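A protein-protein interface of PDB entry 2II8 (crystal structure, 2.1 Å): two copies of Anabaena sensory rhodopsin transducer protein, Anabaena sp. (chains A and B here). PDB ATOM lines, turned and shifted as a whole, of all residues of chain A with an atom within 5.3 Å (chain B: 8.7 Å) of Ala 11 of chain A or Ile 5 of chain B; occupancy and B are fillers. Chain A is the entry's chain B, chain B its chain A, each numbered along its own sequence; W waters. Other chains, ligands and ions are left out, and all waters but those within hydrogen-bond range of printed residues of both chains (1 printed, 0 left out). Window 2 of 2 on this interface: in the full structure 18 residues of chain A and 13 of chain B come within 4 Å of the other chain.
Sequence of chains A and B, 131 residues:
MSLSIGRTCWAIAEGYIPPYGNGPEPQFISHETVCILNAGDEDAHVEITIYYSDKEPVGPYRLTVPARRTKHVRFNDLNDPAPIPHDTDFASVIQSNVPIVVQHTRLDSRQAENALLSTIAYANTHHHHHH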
ATOM      1  N   CYS A   9     -20.847   5.024   3.374  1.00  0.00           N
ATOM      2  CA  CYS A   9     -21.835   5.650   4.214  1.00  0.00           C
ATOM      3  C   CYS A   9     -23.261   5.375   3.692  1.00  0.00           C
ATOM      4  O   CYS A   9     -23.561   5.550   2.499  1.00  0.00           O
ATOM      5  CB  CYS A   9     -21.506   7.147   4.340  1.00  0.00           C
ATOM      6  SG  CYS A   9     -22.656   8.009   5.568  1.00  0.00           S
ATOM      7  N   TRP A  10     -24.122   4.841   4.566  1.00  0.00           N
ATOM      8  CA  TRP A  10     -25.486   4.560   4.254  1.00  0.00           C
ATOM      9  C   TRP A  10     -26.317   5.173   5.394  1.00  0.00           C
ATOM     10  O   TRP A  10     -25.856   5.207   6.588  1.00  0.00           O
ATOM     11  CB  TRP A  10     -25.694   3.048   4.289  1.00  0.00           C
ATOM     12  CG  TRP A  10     -24.914   2.272   3.186  1.00  0.00           C
ATOM     13  CD1 TRP A  10     -23.577   1.869   3.218  1.00  0.00           C
ATOM     14  CD2 TRP A  10     -25.435   1.835   1.932  1.00  0.00           C
ATOM     15  NE1 TRP A  10     -23.259   1.209   2.047  1.00  0.00           N
ATOM     16  CE2 TRP A  10     -24.378   1.179   1.242  1.00  0.00           C
ATOM     17  CE3 TRP A  10     -26.695   1.948   1.307  1.00  0.00           C
ATOM     18  CZ2 TRP A  10     -24.542   0.632  -0.026  1.00  0.00           C
ATOM     19  CZ3 TRP A  10     -26.877   1.377   0.029  1.00  0.00           C
ATOM     20  CH2 TRP A  10     -25.751   0.737  -0.635  1.00  0.00           C
ATOM     21  N   ALA A  11     -27.528   5.615   5.057  1.00  0.00           N
ATOM     22  CA  ALA A  11     -28.464   6.226   6.003  1.00  0.00           C
ATOM     23  C   ALA A  11     -29.802   5.544   5.862  1.00  0.00           C
ATOM     24  O   ALA A  11     -30.289   5.227   4.732  1.00  0.00           O
ATOM     25  CB  ALA A  11     -28.562   7.681   5.727  1.00  0.00           C
ATOM     26  N   ILE A  12     -30.391   5.177   6.991  1.00  0.00           N
ATOM     27  CA  ILE A  12     -31.695   4.555   7.007  1.00  0.00           C
ATOM     28  C   ILE A  12     -32.603   5.504   7.794  1.00  0.00           C
ATOM     29  O   ILE A  12     -32.434   5.637   9.009  1.00  0.00           O
ATOM     30  CB  ILE A  12     -31.619   3.186   7.671  1.00  0.00           C
ATOM     31  CG1 ILE A  12     -30.626   2.313   6.909  1.00  0.00           C
ATOM     32  CG2 ILE A  12     -33.027   2.459   7.704  1.00  0.00           C
ATOM     33  CD1 ILE A  12     -30.460   0.937   7.391  1.00  0.00           C
ATOM     34  N   ALA A  13     -33.597   6.120   7.124  1.00  0.00           N
ATOM     35  CA  ALA A  13     -34.437   7.144   7.764  1.00  0.00           C
ATOM     36  C   ALA A  13     -35.499   6.632   8.723  1.00  0.00           C
ATOM     37  O   ALA A  13     -36.020   7.381   9.519  1.00  0.00           O
ATOM     38  CB  ALA A  13     -35.026   8.064   6.764  1.00  0.00           C
ATOM     39  N   TYR A  51     -30.153   8.152  15.495  1.00  0.00           N
ATOM     40  CA  TYR A  51     -30.719   9.495  15.566  1.00  0.00           C
ATOM     41  C   TYR A  51     -32.130   9.403  16.099  1.00  0.00           C
ATOM     42  O   TYR A  51     -32.837   8.458  15.827  1.00  0.00           O
ATOM     43  CB  TYR A  51     -30.688  10.247  14.188  1.00  0.00           C
ATOM     44  CG  TYR A  51     -29.274  10.571  13.710  1.00  0.00           C
ATOM     45  CD1 TYR A  51     -28.441   9.559  13.115  1.00  0.00           C
ATOM     46  CD2 TYR A  51     -28.771  11.836  13.842  1.00  0.00           C
ATOM     47  CE1 TYR A  51     -27.095   9.889  12.694  1.00  0.00           C
ATOM     48  CE2 TYR A  51     -27.460  12.168  13.416  1.00  0.00           C
ATOM     49  CZ  TYR A  51     -26.651  11.158  12.858  1.00  0.00           C
ATOM     50  OH  TYR A  51     -25.397  11.482  12.460  1.00  0.00           O
ATOM     51  N   SER A  92     -30.784   5.730  11.395  1.00  0.00           N
ATOM     52  CA  SER A  92     -29.330   5.443  11.594  1.00  0.00           C
ATOM     53  C   SER A  92     -28.449   5.815  10.413  1.00  0.00           C
ATOM     54  O   SER A  92     -28.920   5.887   9.271  1.00  0.00           O
ATOM     55  CB  SER A  92     -29.160   3.979  11.849  1.00  0.00           C
ATOM     56  OG  SER A  92     -29.755   3.253  10.787  1.00  0.00           O
ATOM     57  N   VAL A  93     -27.167   6.057  10.692  1.00  0.00           N
ATOM     58  CA  VAL A  93     -26.143   6.257   9.714  1.00  0.00           C
ATOM     59  C   VAL A  93     -25.186   5.100   9.986  1.00  0.00           C
ATOM     60  O   VAL A  93     -24.786   4.823  11.153  1.00  0.00           O
ATOM     61  CB  VAL A  93     -25.481   7.640   9.815  1.00  0.00           C
ATOM     62  CG1 VAL A  93     -24.261   7.776   8.916  1.00  0.00           C
ATOM     63  CG2 VAL A  93     -26.519   8.749   9.453  1.00  0.00           C
ATOM     64  N   ILE A  94     -24.854   4.381   8.916  1.00  0.00           N
ATOM     65  CA  ILE A  94     -23.902   3.286   8.943  1.00  0.00           C
ATOM     66  C   ILE A  94     -22.674   3.677   8.151  1.00  0.00           C
ATOM     67  O   ILE A  94     -22.791   3.959   6.954  1.00  0.00           O
ATOM     68  CB  ILE A  94     -24.557   2.063   8.372  1.00  0.00           C
ATOM     69  CG1 ILE A  94     -25.796   1.802   9.221  1.00  0.00           C
ATOM     70  CG2 ILE A  94     -23.543   0.826   8.303  1.00  0.00           C
ATOM     71  CD1 ILE A  94     -26.958   1.453   8.440  1.00  0.00           C
ATOM     72  N   SER B   2     -20.866  19.161   9.898  1.00  0.00           N
ATOM     73  CA  SER B   2     -19.918  17.985   9.793  1.00  0.00           C
ATOM     74  C   SER B   2     -20.385  16.936   8.765  1.00  0.00           C
ATOM     75  O   SER B   2     -19.986  16.986   7.569  1.00  0.00           O
ATOM     76  CB  SER B   2     -19.713  17.335  11.165  1.00  0.00           C
ATOM     77  OG  SER B   2     -19.132  18.273  12.064  1.00  0.00           O
ATOM     78  N   LEU B   3     -21.232  16.003   9.214  1.00  0.00           N
ATOM     79  CA  LEU B   3     -21.725  14.946   8.323  1.00  0.00           C
ATOM     80  C   LEU B   3     -22.705  15.542   7.301  1.00  0.00           C
ATOM     81  O   LEU B   3     -23.647  16.202   7.690  1.00  0.00           O
ATOM     82  CB  LEU B   3     -22.395  13.832   9.127  1.00  0.00           C
ATOM     83  CG  LEU B   3     -22.538  12.424   8.547  1.00  0.00           C
ATOM     84  CD1 LEU B   3     -21.224  11.805   7.966  1.00  0.00           C
ATOM     85  CD2 LEU B   3     -23.154  11.503   9.621  1.00  0.00           C
ATOM     86  N   SER B   4     -22.460  15.343   6.013  1.00  0.00           N
ATOM     87  CA  SER B   4     -23.458  15.712   4.988  1.00  0.00           C
ATOM     88  C   SER B   4     -23.942  14.456   4.240  1.00  0.00           C
ATOM     89  O   SER B   4     -23.211  13.863   3.429  1.00  0.00           O
ATOM     90  CB  SER B   4     -22.897  16.749   4.000  1.00  0.00           C
ATOM     91  OG  SER B   4     -23.879  17.728   3.695  1.00  0.00           O
ATOM     92  N   ILE B   5     -25.145  14.007   4.543  1.00  0.00           N
ATOM     93  CA  ILE B   5     -25.657  12.817   3.898  1.00  0.00           C
ATOM     94  C   ILE B   5     -27.046  13.180   3.360  1.00  0.00           C
ATOM     95  O   ILE B   5     -27.825  13.813   4.076  1.00  0.00           O
ATOM     96  CB  ILE B   5     -25.911  11.635   4.890  1.00  0.00           C
ATOM     97  CG1 ILE B   5     -24.951  11.691   6.046  1.00  0.00           C
ATOM     98  CG2 ILE B   5     -25.939  10.252   4.150  1.00  0.00           C
ATOM     99  CD1 ILE B   5     -25.423  10.950   7.217  1.00  0.00           C
ATOM    100  N   GLY B   6     -27.326  12.714   2.145  1.00  0.00           N
ATOM    101  CA  GLY B   6     -28.619  12.784   1.526  1.00  0.00           C
ATOM    102  C   GLY B   6     -28.671  13.798   0.423  1.00  0.00           C
ATOM    103  O   GLY B   6     -27.686  14.119  -0.230  1.00  0.00           O
ATOM    104  N   ARG B   7     -29.845  14.382   0.217  1.00  0.00           N
ATOM    105  CA  ARG B   7     -29.972  15.399  -0.802  1.00  0.00           C
ATOM    106  C   ARG B   7     -31.123  16.342  -0.581  1.00  0.00           C
ATOM    107  O   ARG B   7     -31.907  16.136   0.343  1.00  0.00           O
ATOM    108  CB  ARG B   7     -30.182  14.722  -2.138  1.00  0.00           C
ATOM    109  CG  ARG B   7     -31.250  13.754  -2.138  1.00  0.00           C
ATOM    110  CD  ARG B   7     -31.155  13.015  -3.489  1.00  0.00           C
ATOM    111  NE  ARG B   7     -32.384  12.342  -3.801  1.00  0.00           N
ATOM    112  CZ  ARG B   7     -32.499  11.027  -3.884  1.00  0.00           C
ATOM    113  NH1 ARG B   7     -31.456  10.279  -3.674  1.00  0.00           N
ATOM    114  NH2 ARG B   7     -33.657  10.467  -4.187  1.00  0.00           N
ATOM    115  N   THR B   8     -31.183  17.395  -1.377  1.00  0.00           N
ATOM    116  CA  THR B   8     -32.100  18.488  -1.064  1.00  0.00           C
ATOM    117  C   THR B   8     -33.462  18.290  -1.683  1.00  0.00           C
ATOM    118  O   THR B   8     -34.364  19.064  -1.416  1.00  0.00           O
ATOM    119  CB  THR B   8     -31.547  19.870  -1.449  1.00  0.00           C
ATOM    120  OG1 THR B   8     -31.045  19.792  -2.783  1.00  0.00           O
ATOM    121  CG2 THR B   8     -30.294  20.261  -0.539  1.00  0.00           C
ATOM    122  N   TRP B  10     -36.350  15.137  -2.888  1.00  0.00           N
ATOM    123  CA  TRP B  10     -36.776  13.775  -2.937  1.00  0.00           C
ATOM    124  C   TRP B  10     -38.214  13.804  -3.500  1.00  0.00           C
ATOM    125  O   TRP B  10     -38.980  14.686  -3.119  1.00  0.00           O
ATOM    126  CB  TRP B  10     -36.859  13.151  -1.506  1.00  0.00           C
ATOM    127  CG  TRP B  10     -35.504  13.031  -0.825  1.00  0.00           C
ATOM    128  CD1 TRP B  10     -34.803  14.032  -0.242  1.00  0.00           C
ATOM    129  CD2 TRP B  10     -34.698  11.873  -0.741  1.00  0.00           C
ATOM    130  NE1 TRP B  10     -33.619  13.571   0.272  1.00  0.00           N
ATOM    131  CE2 TRP B  10     -33.503  12.250  -0.038  1.00  0.00           C
ATOM    132  CE3 TRP B  10     -34.825  10.562  -1.222  1.00  0.00           C
ATOM    133  CZ2 TRP B  10     -32.461  11.370   0.195  1.00  0.00           C
ATOM    134  CZ3 TRP B  10     -33.791   9.636  -0.929  1.00  0.00           C
ATOM    135  CH2 TRP B  10     -32.629  10.048  -0.204  1.00  0.00           C
ATOM    136  N   LEU B  37     -34.467  12.166   8.018  1.00  0.00           N
ATOM    137  CA  LEU B  37     -33.300  12.277   8.889  1.00  0.00           C
ATOM    138  C   LEU B  37     -32.538  13.459   8.423  1.00  0.00           C
ATOM    139  O   LEU B  37     -32.216  13.569   7.209  1.00  0.00           O
ATOM    140  CB  LEU B  37     -32.439  10.984   8.810  1.00  0.00           C
ATOM    141  CG  LEU B  37     -30.989  11.127   9.311  1.00  0.00           C
ATOM    142  CD1 LEU B  37     -31.014  11.239  10.877  1.00  0.00           C
ATOM    143  CD2 LEU B  37     -30.222   9.885   8.856  1.00  0.00           C
ATOM    144  N   ASN B  38     -32.288  14.393   9.344  1.00  0.00           N
ATOM    145  CA  ASN B  38     -31.331  15.455   9.123  1.00  0.00           C
ATOM    146  C   ASN B  38     -30.068  15.106   9.951  1.00  0.00           C
ATOM    147  O   ASN B  38     -30.041  15.361  11.141  1.00  0.00           O
ATOM    148  CB  ASN B  38     -31.929  16.843   9.494  1.00  0.00           C
ATOM    149  CG  ASN B  38     -30.961  17.912   9.276  1.00  0.00           C
ATOM    150  OD1 ASN B  38     -29.982  17.694   8.756  1.00  0.00           O
ATOM    151  ND2 ASN B  38     -31.204  19.046   9.668  1.00  0.00           N
ATOM    152  N   ALA B  39     -29.052  14.482   9.343  1.00  0.00           N
ATOM    153  CA  ALA B  39     -27.819  14.152  10.075  1.00  0.00           C
ATOM    154  C   ALA B  39     -26.842  15.327  10.097  1.00  0.00           C
ATOM    155  O   ALA B  39     -25.781  15.211  10.685  1.00  0.00           O
ATOM    156  CB  ALA B  39     -27.137  12.917   9.459  1.00  0.00           C
ATOM    157  N   GLY B  40     -27.184  16.440   9.474  1.00  0.00           N
ATOM    158  CA  GLY B  40     -26.315  17.589   9.365  1.00  0.00           C
ATOM    159  C   GLY B  40     -26.421  18.536  10.581  1.00  0.00           C
ATOM    160  O   GLY B  40     -27.314  18.339  11.452  1.00  0.00           O
ATOM    161  N   ASP B  41     -25.565  19.558  10.587  1.00  0.00           N
ATOM    162  CA  ASP B  41     -25.447  20.512  11.724  1.00  0.00           C
ATOM    163  C   ASP B  41     -26.347  21.760  11.631  1.00  0.00           C
ATOM    164  O   ASP B  41     -26.375  22.593  12.563  1.00  0.00           O
ATOM    165  CB  ASP B  41     -23.983  20.949  11.814  1.00  0.00           C
ATOM    166  CG  ASP B  41     -23.094  19.866  12.503  1.00  0.00           C
ATOM    167  OD1 ASP B  41     -23.613  18.888  13.120  1.00  0.00           O
ATOM    168  OD2 ASP B  41     -21.869  19.997  12.381  1.00  0.00           O
ATOM    169  N   VAL B  98     -30.975  22.043   3.049  1.00  0.00           N
ATOM    170  CA  VAL B  98     -29.764  21.275   3.360  1.00  0.00           C
ATOM    171  C   VAL B  98     -30.099  19.832   3.047  1.00  0.00           C
ATOM    172  O   VAL B  98     -31.292  19.434   3.123  1.00  0.00           O
ATOM    173  CB  VAL B  98     -29.359  21.413   4.933  1.00  0.00           C
ATOM    174  CG1 VAL B  98     -29.089  22.849   5.272  1.00  0.00           C
ATOM    175  CG2 VAL B  98     -30.479  20.871   5.829  1.00  0.00           C
ATOM    176  N   PRO B  99     -29.076  18.997   2.723  1.00  0.00           N
ATOM    177  CA  PRO B  99     -29.354  17.581   2.492  1.00  0.00           C
ATOM    178  C   PRO B  99     -30.036  16.889   3.642  1.00  0.00           C
ATOM    179  O   PRO B  99     -29.637  17.076   4.816  1.00  0.00           O
ATOM    180  CB  PRO B  99     -27.968  16.954   2.326  1.00  0.00           C
ATOM    181  CG  PRO B  99     -27.109  18.025   2.001  1.00  0.00           C
ATOM    182  CD  PRO B  99     -27.641  19.314   2.535  1.00  0.00           C
ATOM    183  N   ILE B 100     -30.999  16.022   3.302  1.00  0.00           N
ATOM    184  CA  ILE B 100     -31.702  15.205   4.238  1.00  0.00           C
ATOM    185  C   ILE B 100     -31.872  13.865   3.605  1.00  0.00           C
ATOM    186  O   ILE B 100     -31.677  13.710   2.397  1.00  0.00           O
ATOM    187  CB  ILE B 100     -33.090  15.810   4.583  1.00  0.00           C
ATOM    188  CG1 ILE B 100     -33.904  16.038   3.261  1.00  0.00           C
ATOM    189  CG2 ILE B 100     -32.890  17.122   5.339  1.00  0.00           C
ATOM    190  CD1 ILE B 100     -35.436  16.544   3.470  1.00  0.00           C
ATOM    191  N   VAL B 101     -32.166  12.883   4.414  1.00  0.00           N
ATOM    192  CA  VAL B 101     -32.482  11.551   3.923  1.00  0.00           C
ATOM    193  C   VAL B 101     -33.962  11.306   4.176  1.00  0.00           C
ATOM    194  O   VAL B 101     -34.469  11.576   5.249  1.00  0.00           O
ATOM    195  CB  VAL B 101     -31.645  10.511   4.684  1.00  0.00           C
ATOM    196  CG1 VAL B 101     -31.954   9.120   4.248  1.00  0.00           C
ATOM    197  CG2 VAL B 101     -30.137  10.815   4.454  1.00  0.00           C
ATOM    198  N   VAL B 102     -34.671  10.855   3.149  1.00  0.00           N
ATOM    199  CA  VAL B 102     -36.117  10.637   3.209  1.00  0.00           C
ATOM    200  C   VAL B 102     -36.486   9.198   2.851  1.00  0.00           C
ATOM    201  O   VAL B 102     -36.008   8.697   1.877  1.00  0.00           O
ATOM    202  CB  VAL B 102     -36.904  11.573   2.251  1.00  0.00           C
ATOM    203  CG1 VAL B 102     -38.403  11.159   2.236  1.00  0.00           C
ATOM    204  CG2 VAL B 102     -36.735  13.112   2.644  1.00  0.00           C
ATOM    205  N   GLN B 103     -37.342   8.551   3.632  1.00  0.00           N
ATOM    206  CA  GLN B 103     -37.796   7.222   3.316  1.00  0.00           C
ATOM    207  C   GLN B 103     -39.276   7.287   3.587  1.00  0.00           C
ATOM    208  O   GLN B 103     -39.723   8.061   4.438  1.00  0.00           O
ATOM    209  CB  GLN B 103     -37.142   6.199   4.248  1.00  0.00           C
ATOM    210  CG  GLN B 103     -37.496   4.706   4.094  1.00  0.00           C
ATOM    211  CD  GLN B 103     -36.620   3.793   5.027  1.00  0.00           C
ATOM    212  OE1 GLN B 103     -35.656   4.256   5.645  1.00  0.00           O
ATOM    213  NE2 GLN B 103     -36.966   2.504   5.097  1.00  0.00           N
HETATM  214  O   HOH W   1     -33.660   5.495   4.260  1.00  0.00           O
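The backbone NH (N) of Leu 37 of chain B lies within hydrogen-bond range of the backbone carbonyl oxygen (O) of Val 101 of chain B (2.8 Å).
The backbone carbonyl oxygen of Ser 92 of chain A is in hydrogen-bond range of the backbone NH of Ile 12 of chain A.
Printed residues of chain B within 4 Å of Ala 11 of chain A: Ile 5 (3.997 Å) and Val 101 (3.7 Å).
Of the printed residues of chain B, Ala 13 of chain A touches Val 101 and Gln 103.
Ile 94 of chain A touches none of the printed residues of chain B.
Printed residues of chain A within 4 Å of Ile 5 of chain B: Ala 11 (3.997 Å) and Val 93 (3.3 Å).
Of the printed residues of chain A, Ala 39 of chain B touches Tyr 51.
The nearest printed residue of chain B that does not touch Ala 11 of chain A is Leu 37 of chain B (4.2 Å).
The nearest printed residue of chain A that does not touch Leu 37 of chain B is Ala 11 of chain A (4.2 Å).
Among the printed residues, pairs that only touch across the chains: Ala 11 of chain A with Ile 5 of chain B (3.997 Å), Ala 11 of chain A with Val 101 of chain B (3.7 Å), Ile 12 of chain A with Gln 103 of chain B (3.8 Å), Ala 13 of chain A with Val 101 of chain B (3.9 Å), Tyr 51 of chain A with Leu 3 of chain B (3.6 Å), Tyr 51 of chain A with Leu 37 of chain B (3.4 Å), Tyr 51 of chain A with Ala 39 of chain B (3.8 Å), Val 93 of chain A with Leu 3 of chain B (3.95 Å), Val 93 of chain A with Ile 5 of chain B (3.3 Å) and Val 93 of chain A with Leu 37 of chain B (3.9 Å).
Of the 9 printed residues of chain A, 5 touch a printed residue of chain B.
Hydrophobic or aromatic side chains of chain A that line the printed part of chain B: Ala 11, Ile 12, Ala 13, Tyr 51 and Val 93.
Water W1 lies within hydrogen-bond range of OE1 of Gln 103 of chain B (2.7 Å), N of Ala 13 of chain A (2.9 Å) and O of Ala 11 of chain A (3.4 Å).
The side-chain amide oxygen (OE1) of Gln 103 of chain B sits at hydrogen-bond distance from the backbone NH (N) of Ala 13 of chain A.
1 position is printed for both chains.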
